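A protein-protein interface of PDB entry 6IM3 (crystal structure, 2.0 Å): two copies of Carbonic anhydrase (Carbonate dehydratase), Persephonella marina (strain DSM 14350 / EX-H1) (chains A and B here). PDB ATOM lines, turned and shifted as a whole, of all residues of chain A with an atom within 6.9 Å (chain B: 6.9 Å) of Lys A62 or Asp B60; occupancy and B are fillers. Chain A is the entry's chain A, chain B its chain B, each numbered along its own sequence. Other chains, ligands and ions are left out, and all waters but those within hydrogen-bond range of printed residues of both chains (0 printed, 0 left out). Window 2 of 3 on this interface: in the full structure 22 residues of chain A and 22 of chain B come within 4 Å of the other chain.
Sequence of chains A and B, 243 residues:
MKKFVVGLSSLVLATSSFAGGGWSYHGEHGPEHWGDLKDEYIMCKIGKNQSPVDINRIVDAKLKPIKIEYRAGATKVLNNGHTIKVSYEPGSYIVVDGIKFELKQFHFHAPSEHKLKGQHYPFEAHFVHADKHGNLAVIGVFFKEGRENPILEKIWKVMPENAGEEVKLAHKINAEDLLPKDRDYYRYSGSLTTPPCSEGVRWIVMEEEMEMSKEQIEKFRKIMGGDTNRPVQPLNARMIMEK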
ATOM      1  N   VAL A  59      33.047  12.738  27.827  1.00  0.00           N
ATOM      2  CA  VAL A  59      33.186  14.084  27.369  1.00  0.00           C
ATOM      3  C   VAL A  59      33.277  15.018  28.529  1.00  0.00           C
ATOM      4  O   VAL A  59      32.525  14.880  29.464  1.00  0.00           O
ATOM      5  CB  VAL A  59      32.037  14.402  26.373  1.00  0.00           C
ATOM      6  CG1 VAL A  59      30.702  14.425  27.073  1.00  0.00           C
ATOM      7  CG2 VAL A  59      32.274  15.713  25.693  1.00  0.00           C
ATOM      8  N   ASP A  60      34.137  16.019  28.432  1.00  0.00           N
ATOM      9  CA  ASP A  60      34.222  17.065  29.396  1.00  0.00           C
ATOM     10  C   ASP A  60      32.906  17.872  29.349  1.00  0.00           C
ATOM     11  O   ASP A  60      32.428  18.230  28.294  1.00  0.00           O
ATOM     12  CB  ASP A  60      35.315  18.110  29.100  1.00  0.00           C
ATOM     13  CG  ASP A  60      36.759  17.556  29.208  1.00  0.00           C
ATOM     14  OD1 ASP A  60      36.942  16.394  29.530  1.00  0.00           O
ATOM     15  OD2 ASP A  60      37.708  18.348  28.983  1.00  0.00           O
ATOM     16  N   ALA A  61      32.386  18.213  30.525  1.00  0.00           N
ATOM     17  CA  ALA A  61      31.155  18.965  30.623  1.00  0.00           C
ATOM     18  C   ALA A  61      31.199  19.894  31.783  1.00  0.00           C
ATOM     19  O   ALA A  61      31.773  19.571  32.825  1.00  0.00           O
ATOM     20  CB  ALA A  61      29.961  18.005  30.729  1.00  0.00           C
ATOM     21  N   LYS A  62      30.490  20.999  31.665  1.00  0.00           N
ATOM     22  CA  LYS A  62      30.481  22.021  32.707  1.00  0.00           C
ATOM     23  C   LYS A  62      29.457  21.700  33.785  1.00  0.00           C
ATOM     24  O   LYS A  62      28.482  22.384  33.934  1.00  0.00           O
ATOM     25  CB  LYS A  62      30.151  23.409  32.157  1.00  0.00           C
ATOM     26  CG  LYS A  62      31.259  24.072  31.379  1.00  0.00           C
ATOM     27  CD  LYS A  62      30.911  25.584  31.199  1.00  0.00           C
ATOM     28  CE  LYS A  62      31.940  26.346  30.376  1.00  0.00           C
ATOM     29  NZ  LYS A  62      31.810  26.091  28.914  1.00  0.00           N
ATOM     30  N   LEU A  63      29.673  20.630  34.502  1.00  0.00           N
ATOM     31  CA  LEU A  63      28.718  20.210  35.516  1.00  0.00           C
ATOM     32  C   LEU A  63      28.940  20.974  36.805  1.00  0.00           C
ATOM     33  O   LEU A  63      30.057  21.353  37.124  1.00  0.00           O
ATOM     34  CB  LEU A  63      28.913  18.695  35.773  1.00  0.00           C
ATOM     35  CG  LEU A  63      28.670  17.793  34.566  1.00  0.00           C
ATOM     36  CD1 LEU A  63      29.218  16.385  34.774  1.00  0.00           C
ATOM     37  CD2 LEU A  63      27.189  17.778  34.279  1.00  0.00           C
ATOM     38  N   LYS A  64      27.896  21.118  37.571  1.00  0.00           N
ATOM     39  CA  LYS A  64      27.990  21.754  38.857  1.00  0.00           C
ATOM     40  C   LYS A  64      28.508  20.770  39.907  1.00  0.00           C
ATOM     41  O   LYS A  64      28.244  19.609  39.817  1.00  0.00           O
ATOM     42  CB  LYS A  64      26.620  22.199  39.380  1.00  0.00           C
ATOM     43  CG  LYS A  64      25.861  23.120  38.495  1.00  0.00           C
ATOM     44  CD  LYS A  64      24.631  23.620  39.251  1.00  0.00           C
ATOM     45  CE  LYS A  64      23.504  23.913  38.264  1.00  0.00           C
ATOM     46  NZ  LYS A  64      22.339  24.550  38.930  1.00  0.00           N
ATOM     47  N   TYR A 185      33.522  14.133  39.279  1.00  0.00           N
ATOM     48  CA  TYR A 185      32.722  12.979  39.035  1.00  0.00           C
ATOM     49  C   TYR A 185      32.360  12.768  37.559  1.00  0.00           C
ATOM     50  O   TYR A 185      32.390  13.722  36.794  1.00  0.00           O
ATOM     51  CB  TYR A 185      31.462  13.013  39.880  1.00  0.00           C
ATOM     52  CG  TYR A 185      30.546  14.145  39.584  1.00  0.00           C
ATOM     53  CD1 TYR A 185      30.664  15.391  40.231  1.00  0.00           C
ATOM     54  CD2 TYR A 185      29.509  13.995  38.612  1.00  0.00           C
ATOM     55  CE1 TYR A 185      29.790  16.432  39.901  1.00  0.00           C
ATOM     56  CE2 TYR A 185      28.634  15.038  38.300  1.00  0.00           C
ATOM     57  CZ  TYR A 185      28.765  16.245  38.941  1.00  0.00           C
ATOM     58  OH  TYR A 185      27.881  17.264  38.643  1.00  0.00           O
ATOM     59  N   GLU A 242      31.952  14.145  32.206  1.00  0.00           N
ATOM     60  CA  GLU A 242      32.971  14.343  33.254  1.00  0.00           C
ATOM     61  C   GLU A 242      33.049  15.774  33.696  1.00  0.00           C
ATOM     62  O   GLU A 242      33.238  16.678  32.886  1.00  0.00           O
ATOM     63  CB  GLU A 242      34.337  13.920  32.767  1.00  0.00           C
ATOM     64  CG  GLU A 242      35.341  13.928  33.879  1.00  0.00           C
ATOM     65  CD  GLU A 242      36.788  13.731  33.426  1.00  0.00           C
ATOM     66  OE1 GLU A 242      37.027  13.281  32.275  1.00  0.00           O
ATOM     67  OE2 GLU A 242      37.671  14.052  34.269  1.00  0.00           O
ATOM     68  N   LYS A 243      32.969  15.973  35.009  1.00  0.00           N
ATOM     69  CA  LYS A 243      33.071  17.358  35.570  1.00  0.00           C
ATOM     70  C   LYS A 243      34.459  18.105  35.500  1.00  0.00           C
ATOM     71  O   LYS A 243      35.479  17.460  35.748  1.00  0.00           O
ATOM     72  CB  LYS A 243      32.650  17.338  37.004  1.00  0.00           C
ATOM     73  CG  LYS A 243      32.738  18.737  37.581  1.00  0.00           C
ATOM     74  CD  LYS A 243      32.345  18.799  39.019  1.00  0.00           C
ATOM     75  CE  LYS A 243      32.311  20.254  39.484  1.00  0.00           C
ATOM     76  NZ  LYS A 243      33.680  20.750  39.689  1.00  0.00           N
ATOM     77  N   ILE B  58      20.426  21.928  30.421  1.00  0.00           N
ATOM     78  CA  ILE B  58      21.457  21.880  29.425  1.00  0.00           C
ATOM     79  C   ILE B  58      22.815  22.130  30.073  1.00  0.00           C
ATOM     80  O   ILE B  58      22.941  23.006  30.886  1.00  0.00           O
ATOM     81  CB  ILE B  58      21.231  22.975  28.365  1.00  0.00           C
ATOM     82  CG1 ILE B  58      19.826  22.862  27.789  1.00  0.00           C
ATOM     83  CG2 ILE B  58      22.247  22.855  27.255  1.00  0.00           C
ATOM     84  CD1 ILE B  58      19.399  24.096  26.995  1.00  0.00           C
ATOM     85  N   VAL B  59      23.808  21.434  29.609  1.00  0.00           N
ATOM     86  CA  VAL B  59      25.175  21.643  30.046  1.00  0.00           C
ATOM     87  C   VAL B  59      26.117  21.740  28.848  1.00  0.00           C
ATOM     88  O   VAL B  59      25.983  20.970  27.907  1.00  0.00           O
ATOM     89  CB  VAL B  59      25.573  20.523  31.050  1.00  0.00           C
ATOM     90  CG1 VAL B  59      25.676  19.184  30.386  1.00  0.00           C
ATOM     91  CG2 VAL B  59      26.922  20.862  31.667  1.00  0.00           C
ATOM     92  N   ASP B  60      27.018  22.715  28.861  1.00  0.00           N
ATOM     93  CA  ASP B  60      28.039  22.824  27.848  1.00  0.00           C
ATOM     94  C   ASP B  60      28.951  21.575  27.907  1.00  0.00           C
ATOM     95  O   ASP B  60      29.357  21.142  28.989  1.00  0.00           O
ATOM     96  CB  ASP B  60      29.010  24.030  28.103  1.00  0.00           C
ATOM     97  CG  ASP B  60      28.344  25.407  27.962  1.00  0.00           C
ATOM     98  OD1 ASP B  60      27.194  25.505  27.625  1.00  0.00           O
ATOM     99  OD2 ASP B  60      29.052  26.410  28.173  1.00  0.00           O
ATOM    100  N   ALA B  61      29.276  21.034  26.764  1.00  0.00           N
ATOM    101  CA  ALA B  61      30.085  19.878  26.684  1.00  0.00           C
ATOM    102  C   ALA B  61      31.032  19.972  25.495  1.00  0.00           C
ATOM    103  O   ALA B  61      30.630  20.431  24.436  1.00  0.00           O
ATOM    104  CB  ALA B  61      29.221  18.628  26.618  1.00  0.00           C
ATOM    105  N   LYS B  62      32.190  19.320  25.599  1.00  0.00           N
ATOM    106  CA  LYS B  62      33.161  19.340  24.528  1.00  0.00           C
ATOM    107  C   LYS B  62      32.914  18.295  23.473  1.00  0.00           C
ATOM    108  O   LYS B  62      33.620  17.339  23.373  1.00  0.00           O
ATOM    109  CB  LYS B  62      34.593  19.149  25.077  1.00  0.00           C
ATOM    110  CG  LYS B  62      35.166  20.322  25.800  1.00  0.00           C
ATOM    111  CD  LYS B  62      36.685  20.108  25.960  1.00  0.00           C
ATOM    112  CE  LYS B  62      37.374  21.207  26.733  1.00  0.00           C
ATOM    113  NZ  LYS B  62      37.181  21.043  28.208  1.00  0.00           N
ATOM    114  N   LEU B  63      31.792  18.401  22.786  1.00  0.00           N
ATOM    115  CA  LEU B  63      31.418  17.368  21.842  1.00  0.00           C
ATOM    116  C   LEU B  63      32.128  17.596  20.525  1.00  0.00           C
ATOM    117  O   LEU B  63      32.413  18.721  20.152  1.00  0.00           O
ATOM    118  CB  LEU B  63      29.885  17.427  21.629  1.00  0.00           C
ATOM    119  CG  LEU B  63      29.022  17.139  22.833  1.00  0.00           C
ATOM    120  CD1 LEU B  63      27.573  17.588  22.644  1.00  0.00           C
ATOM    121  CD2 LEU B  63      29.100  15.669  23.137  1.00  0.00           C
ATOM    122  N   ILE B 240      20.865  17.318  28.892  1.00  0.00           N
ATOM    123  CA  ILE B 240      21.072  17.508  27.472  1.00  0.00           C
ATOM    124  C   ILE B 240      22.465  18.157  27.359  1.00  0.00           C
ATOM    125  O   ILE B 240      22.758  19.134  28.085  1.00  0.00           O
ATOM    126  CB  ILE B 240      20.054  18.483  26.898  1.00  0.00           C
ATOM    127  CG1 ILE B 240      18.632  18.222  27.353  1.00  0.00           C
ATOM    128  CG2 ILE B 240      20.232  18.559  25.403  1.00  0.00           C
ATOM    129  CD1 ILE B 240      18.114  16.955  26.975  1.00  0.00           C
ATOM    130  N   MET B 241      23.305  17.654  26.499  1.00  0.00           N
ATOM    131  CA  MET B 241      24.611  18.220  26.293  1.00  0.00           C
ATOM    132  C   MET B 241      24.548  19.164  25.109  1.00  0.00           C
ATOM    133  O   MET B 241      23.933  18.840  24.091  1.00  0.00           O
ATOM    134  CB  MET B 241      25.584  17.113  25.950  1.00  0.00           C
ATOM    135  CG  MET B 241      25.814  16.233  27.163  1.00  0.00           C
ATOM    136  SD  MET B 241      26.749  14.754  26.782  1.00  0.00           S
ATOM    137  CE  MET B 241      25.685  13.898  25.583  1.00  0.00           C
ATOM    138  N   GLU B 242      25.202  20.305  25.233  1.00  0.00           N
ATOM    139  CA  GLU B 242      25.311  21.262  24.128  1.00  0.00           C
ATOM    140  C   GLU B 242      26.732  21.421  23.629  1.00  0.00           C
ATOM    141  O   GLU B 242      27.649  21.698  24.421  1.00  0.00           O
ATOM    142  CB  GLU B 242      24.778  22.619  24.562  1.00  0.00           C
ATOM    143  CG  GLU B 242      24.750  23.583  23.408  1.00  0.00           C
ATOM    144  CD  GLU B 242      24.467  25.041  23.808  1.00  0.00           C
ATOM    145  OE1 GLU B 242      24.019  25.292  24.970  1.00  0.00           O
ATOM    146  OE2 GLU B 242      24.781  25.896  22.962  1.00  0.00           O
ATOM    147  N   LYS B 243      26.914  21.306  22.320  1.00  0.00           N
ATOM    148  CA  LYS B 243      28.248  21.478  21.722  1.00  0.00           C
ATOM    149  C   LYS B 243      28.888  22.924  21.773  1.00  0.00           C
ATOM    150  O   LYS B 243      28.213  23.893  21.481  1.00  0.00           O
ATOM    151  CB  LYS B 243      28.230  21.019  20.310  1.00  0.00           C
ATOM    152  CG  LYS B 243      29.601  21.187  19.680  1.00  0.00           C
ATOM    153  CD  LYS B 243      29.648  20.741  18.269  1.00  0.00           C
ATOM    154  CE  LYS B 243      31.069  20.814  17.751  1.00  0.00           C
ATOM    155  NZ  LYS B 243      31.459  22.209  17.463  1.00  0.00           N
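N of Lys B62 is in hydrogen-bond range of O of Asp A60, 2.9 Å away. The backbone NH (N) of Lys A62 sits at hydrogen-bond distance from the backbone carbonyl oxygen (O) of Asp B60, 2.9 Å away.
N of Ala B61 is in hydrogen-bond range of O of Glu B242, 2.9 Å away. N of Ala A61 sits at hydrogen-bond distance from O of Glu A242. O of Val A59 lies within hydrogen-bond range of N of Glu A242. The backbone carbonyl oxygen (O) of Val B59 lies within hydrogen-bond range of the backbone NH (N) of Glu B242 (2.9 Å). The backbone carbonyl oxygen of Ile B240 sits at hydrogen-bond distance from the backbone NH of Val B59 (3.0 Å).
Among the printed residues, merely in contact across the chains: Val A59 with Lys B62 (3.1 Å), Val A59 with Leu B63 (3.99 Å), Val A59 with Met B241 (3.98 Å), Asp A60 with Ala B61 (3.3 Å), Ala A61 with Asp B60 (3.3 Å), Lys A62 with Val B59 (3.1 Å) and Leu A63 with Val B59 (3.96 Å).
Of the printed residues of chain B, Asp A60 touches Ala B61 and Lys B62. Of chain B, only Val B59 and Asp B60 come within 4 Å of Lys A62. Of the printed residues of chain A, Val B59 touches Lys A62 and Leu A63. Asp B60 touches just these residues of chain A: Ala A61 and Lys A62. Of the printed residues of chain A, Ala B61 touches Asp A60 (3.3 Å). Of the printed residues of chain A, Lys B62 touches Val A59 and Asp A60. The nearest residue of chain B that does not touch Lys A62 is Ala B61 (5.0 Å). The nearest residue of chain A that does not touch Asp B60 is Asp A60 (4.3 Å). The nearest printed residue of chain A that does not touch Met B241 is Ala A61 (5.7 Å).
Hydrophobic or aromatic side chains of chain A that line the printed part of chain B: Val A59 and Ala A61. Of the 10 printed residues of chain B, 6 touch a printed residue of chain A. Hydrophobic or aromatic side chains of chain B within 4 Å of the printed part of chain A: Val B59, Ala B61 and Met B241. Among the printed residues, 9 pairs touch across the chains. Among the printed residues, Asp or Glu carboxylates within 4 Å of a Lys or Arg side-chain nitrogen of the other chain: Asp A60 with Lys B62 and Lys A62 with Asp B60.
Val A59 touches Lys B62, and with the chains exchanged Lys A62 touches Val B59. Val A59 touches Leu B63, and with the chains exchanged Leu A63 touches Val B59. Asp A60 touches Ala B61, and with the chains exchanged Ala A61 touches Asp B60. Asp A60 touches Lys B62, and with the chains exchanged Lys A62 touches Asp B60. Positions printed for both chains: 59, 60, 61, 62, 63, 242 and 243.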
